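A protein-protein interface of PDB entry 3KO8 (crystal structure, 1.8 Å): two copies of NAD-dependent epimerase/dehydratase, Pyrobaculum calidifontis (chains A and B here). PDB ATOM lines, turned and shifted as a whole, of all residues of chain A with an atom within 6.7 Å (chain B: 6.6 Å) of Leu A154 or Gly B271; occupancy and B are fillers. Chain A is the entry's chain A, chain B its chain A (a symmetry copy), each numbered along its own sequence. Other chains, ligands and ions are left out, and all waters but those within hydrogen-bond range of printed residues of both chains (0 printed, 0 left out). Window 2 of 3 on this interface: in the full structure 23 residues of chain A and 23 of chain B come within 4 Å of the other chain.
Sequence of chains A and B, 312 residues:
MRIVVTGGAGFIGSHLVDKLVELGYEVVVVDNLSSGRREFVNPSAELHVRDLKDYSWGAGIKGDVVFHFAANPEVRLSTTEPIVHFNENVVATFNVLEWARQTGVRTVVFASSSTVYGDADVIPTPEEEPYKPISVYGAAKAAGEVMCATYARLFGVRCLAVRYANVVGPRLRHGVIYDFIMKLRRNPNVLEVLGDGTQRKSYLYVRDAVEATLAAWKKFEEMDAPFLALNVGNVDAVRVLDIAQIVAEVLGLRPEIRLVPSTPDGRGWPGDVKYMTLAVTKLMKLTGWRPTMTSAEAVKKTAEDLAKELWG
The side-chain hydroxyl (OG1) of Thr A150 sits close to the backbone carbonyl oxygen (O) of Pro B133 (3.3 Å).
NH2 of Arg A153 lies within hydrogen-bond range of O of Pro B133 (3.0 Å).
NH2 of Arg A153 sits at hydrogen-bond distance from OG1 of Thr A150, at 3.5 Å.
Among the printed residues, pairs that only touch across the chains: Thr A150 with Ser B135, Leu A154 with Ile B134, Leu A154 with Gly B271 and Phe A155 with Val B136.
Leu A154 touches just these residues of chain B: Ile B134 and Gly B271.
Gly B271 touches one residue of chain A.
Printed residues of chain A within 4 Å of Val B136: Phe A155 (3.998 Å).
Printed residues of chain A within 4 Å of Pro B133: Thr A150 (3.2 Å) and Arg A153 (3.0 Å).
Of the printed residues of chain B, Arg A153 touches Pro B133.
Val B273 touches none of the printed residues of chain A.
Of the 10 printed residues of chain B, 5 touch a printed residue of chain A.
Hydrophobic or aromatic side chains of chain B that line the printed part of chain A: Pro B133 and Val B136.
Of the 9 printed residues of chain A, 4 touch a printed residue of chain B.
Hydrophobic or aromatic side chains of chain A that line the printed part of chain B: Leu A154 and Phe A155.
No position is printed for both chains.
Of the 6 pairs that touch across the chains among the printed residues, none has its exchanged pair printed and touching as well.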
ATOM      1  N   ALA A 149     -12.533   0.470   6.191  1.00  0.00           N
ATOM      2  CA  ALA A 149     -13.034  -0.824   5.702  1.00  0.00           C
ATOM      3  C   ALA A 149     -14.309  -0.625   4.874  1.00  0.00           C
ATOM      4  O   ALA A 149     -14.503  -1.285   3.839  1.00  0.00           O
ATOM      5  CB  ALA A 149     -13.275  -1.760   6.882  1.00  0.00           C
ATOM      6  N   THR A 150     -15.163   0.316   5.289  1.00  0.00           N
ATOM      7  CA  THR A 150     -16.389   0.606   4.546  1.00  0.00           C
ATOM      8  C   THR A 150     -16.071   1.258   3.196  1.00  0.00           C
ATOM      9  O   THR A 150     -16.675   0.918   2.180  1.00  0.00           O
ATOM     10  CB  THR A 150     -17.320   1.520   5.371  1.00  0.00           C
ATOM     11  OG1 THR A 150     -17.707   0.807   6.559  1.00  0.00           O
ATOM     12  CG2 THR A 150     -18.578   1.899   4.589  1.00  0.00           C
ATOM     13  N   TYR A 151     -15.120   2.185   3.163  1.00  0.00           N
ATOM     14  CA  TYR A 151     -14.779   2.805   1.874  1.00  0.00           C
ATOM     15  C   TYR A 151     -14.166   1.762   0.933  1.00  0.00           C
ATOM     16  O   TYR A 151     -14.292   1.889  -0.301  1.00  0.00           O
ATOM     17  CB  TYR A 151     -13.808   3.978   2.070  1.00  0.00           C
ATOM     18  CG  TYR A 151     -14.514   5.300   2.291  1.00  0.00           C
ATOM     19  CD1 TYR A 151     -15.430   5.466   3.350  1.00  0.00           C
ATOM     20  CD2 TYR A 151     -14.324   6.370   1.404  1.00  0.00           C
ATOM     21  CE1 TYR A 151     -16.149   6.640   3.505  1.00  0.00           C
ATOM     22  CE2 TYR A 151     -15.027   7.553   1.551  1.00  0.00           C
ATOM     23  CZ  TYR A 151     -15.954   7.688   2.597  1.00  0.00           C
ATOM     24  OH  TYR A 151     -16.727   8.822   2.664  1.00  0.00           O
ATOM     25  N   ALA A 152     -13.506   0.757   1.495  1.00  0.00           N
ATOM     26  CA  ALA A 152     -12.930  -0.320   0.683  1.00  0.00           C
ATOM     27  C   ALA A 152     -14.074  -1.139   0.096  1.00  0.00           C
ATOM     28  O   ALA A 152     -14.097  -1.438  -1.106  1.00  0.00           O
ATOM     29  CB  ALA A 152     -12.033  -1.211   1.519  1.00  0.00           C
ATOM     30  N   ARG A 153     -15.032  -1.521   0.938  1.00  0.00           N
ATOM     31  CA  ARG A 153     -16.157  -2.308   0.440  1.00  0.00           C
ATOM     32  C   ARG A 153     -17.086  -1.585  -0.515  1.00  0.00           C
ATOM     33  O   ARG A 153     -17.525  -2.166  -1.533  1.00  0.00           O
ATOM     34  CB  ARG A 153     -16.974  -2.855   1.616  1.00  0.00           C
ATOM     35  CG  ARG A 153     -16.272  -3.966   2.384  1.00  0.00           C
ATOM     36  CD  ARG A 153     -17.176  -4.567   3.454  1.00  0.00           C
ATOM     37  NE  ARG A 153     -17.422  -3.609   4.510  1.00  0.00           N
ATOM     38  CZ  ARG A 153     -16.763  -3.567   5.663  1.00  0.00           C
ATOM     39  NH1 ARG A 153     -15.801  -4.444   5.937  1.00  0.00           N
ATOM     40  NH2 ARG A 153     -17.053  -2.617   6.531  1.00  0.00           N
ATOM     41  N   LEU A 154     -17.384  -0.317  -0.224  1.00  0.00           N
ATOM     42  CA  LEU A 154     -18.323   0.464  -1.018  1.00  0.00           C
ATOM     43  C   LEU A 154     -17.759   1.200  -2.234  1.00  0.00           C
ATOM     44  O   LEU A 154     -18.354   1.157  -3.324  1.00  0.00           O
ATOM     45  CB  LEU A 154     -19.056   1.473  -0.101  1.00  0.00           C
ATOM     46  CG  LEU A 154     -20.002   2.531  -0.705  1.00  0.00           C
ATOM     47  CD1 LEU A 154     -21.173   1.779  -1.393  1.00  0.00           C
ATOM     48  CD2 LEU A 154     -20.558   3.488   0.377  1.00  0.00           C
ATOM     49  N   PHE A 155     -16.607   1.846  -2.065  1.00  0.00           N
ATOM     50  CA  PHE A 155     -16.024   2.631  -3.144  1.00  0.00           C
ATOM     51  C   PHE A 155     -14.788   2.009  -3.807  1.00  0.00           C
ATOM     52  O   PHE A 155     -14.237   2.578  -4.750  1.00  0.00           O
ATOM     53  CB  PHE A 155     -15.694   4.028  -2.623  1.00  0.00           C
ATOM     54  CG  PHE A 155     -16.871   4.760  -2.061  1.00  0.00           C
ATOM     55  CD1 PHE A 155     -17.943   5.111  -2.878  1.00  0.00           C
ATOM     56  CD2 PHE A 155     -16.904   5.138  -0.720  1.00  0.00           C
ATOM     57  CE1 PHE A 155     -19.028   5.834  -2.374  1.00  0.00           C
ATOM     58  CE2 PHE A 155     -17.974   5.860  -0.214  1.00  0.00           C
ATOM     59  CZ  PHE A 155     -19.041   6.212  -1.034  1.00  0.00           C
ATOM     60  N   GLY A 156     -14.342   0.866  -3.313  1.00  0.00           N
ATOM     61  CA  GLY A 156     -13.197   0.223  -3.919  1.00  0.00           C
ATOM     62  C   GLY A 156     -11.866   0.829  -3.548  1.00  0.00           C
ATOM     63  O   GLY A 156     -10.846   0.516  -4.170  1.00  0.00           O
ATOM     64  N   VAL A 157     -11.857   1.705  -2.543  1.00  0.00           N
ATOM     65  CA  VAL A 157     -10.592   2.304  -2.074  1.00  0.00           C
ATOM     66  C   VAL A 157     -10.052   1.272  -1.096  1.00  0.00           C
ATOM     67  O   VAL A 157     -10.431   1.277   0.082  1.00  0.00           O
ATOM     68  CB  VAL A 157     -10.875   3.628  -1.316  1.00  0.00           C
ATOM     69  CG1 VAL A 157      -9.568   4.182  -0.740  1.00  0.00           C
ATOM     70  CG2 VAL A 157     -11.512   4.633  -2.253  1.00  0.00           C
ATOM     71  N   LEU B  77     -29.572   6.274   1.142  1.00  0.00           N
ATOM     72  CA  LEU B  77     -28.226   6.496   1.646  1.00  0.00           C
ATOM     73  C   LEU B  77     -27.229   6.898   0.556  1.00  0.00           C
ATOM     74  O   LEU B  77     -26.382   7.792   0.752  1.00  0.00           O
ATOM     75  CB  LEU B  77     -27.744   5.241   2.395  1.00  0.00           C
ATOM     76  CG  LEU B  77     -28.666   4.737   3.527  1.00  0.00           C
ATOM     77  CD1 LEU B  77     -28.075   3.497   4.239  1.00  0.00           C
ATOM     78  CD2 LEU B  77     -28.903   5.875   4.501  1.00  0.00           C
ATOM     79  N   SER B  78     -27.323   6.253  -0.603  1.00  0.00           N
ATOM     80  CA  SER B  78     -26.383   6.580  -1.672  1.00  0.00           C
ATOM     81  C   SER B  78     -26.594   7.947  -2.319  1.00  0.00           C
ATOM     82  O   SER B  78     -25.733   8.394  -3.086  1.00  0.00           O
ATOM     83  CB  SER B  78     -26.410   5.497  -2.756  1.00  0.00           C
ATOM     84  OG  SER B  78     -27.575   5.618  -3.565  1.00  0.00           O
ATOM     85  N   THR B 115     -27.913  -1.614   9.953  1.00  0.00           N
ATOM     86  CA  THR B 115     -26.875  -1.372   8.932  1.00  0.00           C
ATOM     87  C   THR B 115     -25.442  -1.541   9.430  1.00  0.00           C
ATOM     88  O   THR B 115     -24.519  -1.649   8.626  1.00  0.00           O
ATOM     89  CB  THR B 115     -27.014   0.045   8.268  1.00  0.00           C
ATOM     90  OG1 THR B 115     -26.927   1.078   9.266  1.00  0.00           O
ATOM     91  CG2 THR B 115     -28.355   0.126   7.534  1.00  0.00           C
ATOM     92  N   PRO B 133     -20.295  -2.739   7.823  1.00  0.00           N
ATOM     93  CA  PRO B 133     -21.179  -1.850   7.065  1.00  0.00           C
ATOM     94  C   PRO B 133     -20.766  -1.608   5.617  1.00  0.00           C
ATOM     95  O   PRO B 133     -19.585  -1.583   5.288  1.00  0.00           O
ATOM     96  CB  PRO B 133     -21.200  -0.552   7.903  1.00  0.00           C
ATOM     97  CG  PRO B 133     -19.825  -0.560   8.566  1.00  0.00           C
ATOM     98  CD  PRO B 133     -19.618  -2.036   8.930  1.00  0.00           C
ATOM     99  N   ILE B 134     -21.762  -1.440   4.762  1.00  0.00           N
ATOM    100  CA  ILE B 134     -21.495  -1.194   3.347  1.00  0.00           C
ATOM    101  C   ILE B 134     -21.978   0.192   2.914  1.00  0.00           C
ATOM    102  O   ILE B 134     -21.883   0.537   1.739  1.00  0.00           O
ATOM    103  CB  ILE B 134     -22.133  -2.275   2.459  1.00  0.00           C
ATOM    104  CG1 ILE B 134     -23.628  -2.388   2.753  1.00  0.00           C
ATOM    105  CG2 ILE B 134     -21.420  -3.643   2.712  1.00  0.00           C
ATOM    106  CD1 ILE B 134     -24.445  -3.080   1.650  1.00  0.00           C
ATOM    107  N   SER B 135     -22.519   0.973   3.849  1.00  0.00           N
ATOM    108  CA  SER B 135     -22.937   2.349   3.560  1.00  0.00           C
ATOM    109  C   SER B 135     -22.168   3.275   4.503  1.00  0.00           C
ATOM    110  O   SER B 135     -21.725   2.842   5.572  1.00  0.00           O
ATOM    111  CB  SER B 135     -24.448   2.550   3.767  1.00  0.00           C
ATOM    112  OG  SER B 135     -24.838   2.301   5.119  1.00  0.00           O
ATOM    113  N   VAL B 136     -21.967   4.524   4.101  1.00  0.00           N
ATOM    114  CA  VAL B 136     -21.274   5.447   4.984  1.00  0.00           C
ATOM    115  C   VAL B 136     -22.136   5.604   6.259  1.00  0.00           C
ATOM    116  O   VAL B 136     -21.602   5.756   7.380  1.00  0.00           O
ATOM    117  CB  VAL B 136     -21.090   6.806   4.304  1.00  0.00           C
ATOM    118  CG1 VAL B 136     -20.472   7.819   5.298  1.00  0.00           C
ATOM    119  CG2 VAL B 136     -20.148   6.618   3.055  1.00  0.00           C
ATOM    120  N   GLY B 271     -24.675   0.504  -1.665  1.00  0.00           N
ATOM    121  CA  GLY B 271     -24.617   0.555  -0.209  1.00  0.00           C
ATOM    122  C   GLY B 271     -25.903   0.146   0.485  1.00  0.00           C
ATOM    123  O   GLY B 271     -25.999   0.172   1.721  1.00  0.00           O
ATOM    124  N   ASP B 272     -26.912  -0.248  -0.286  1.00  0.00           N
ATOM    125  CA  ASP B 272     -28.173  -0.654   0.331  1.00  0.00           C
ATOM    126  C   ASP B 272     -28.125  -2.157   0.600  1.00  0.00           C
ATOM    127  O   ASP B 272     -27.898  -2.966  -0.306  1.00  0.00           O
ATOM    128  CB  ASP B 272     -29.362  -0.281  -0.576  1.00  0.00           C
ATOM    129  CG  ASP B 272     -30.727  -0.764  -0.037  1.00  0.00           C
ATOM    130  OD1 ASP B 272     -31.061  -0.548   1.160  1.00  0.00           O
ATOM    131  OD2 ASP B 272     -31.492  -1.364  -0.834  1.00  0.00           O
ATOM    132  N   VAL B 273     -28.299  -2.517   1.867  1.00  0.00           N
ATOM    133  CA  VAL B 273     -28.311  -3.913   2.278  1.00  0.00           C
ATOM    134  C   VAL B 273     -29.542  -4.566   1.648  1.00  0.00           C
ATOM    135  O   VAL B 273     -30.638  -4.039   1.735  1.00  0.00           O
ATOM    136  CB  VAL B 273     -28.384  -4.041   3.817  1.00  0.00           C
ATOM    137  CG1 VAL B 273     -28.592  -5.528   4.204  1.00  0.00           C
ATOM    138  CG2 VAL B 273     -27.110  -3.493   4.436  1.00  0.00           C
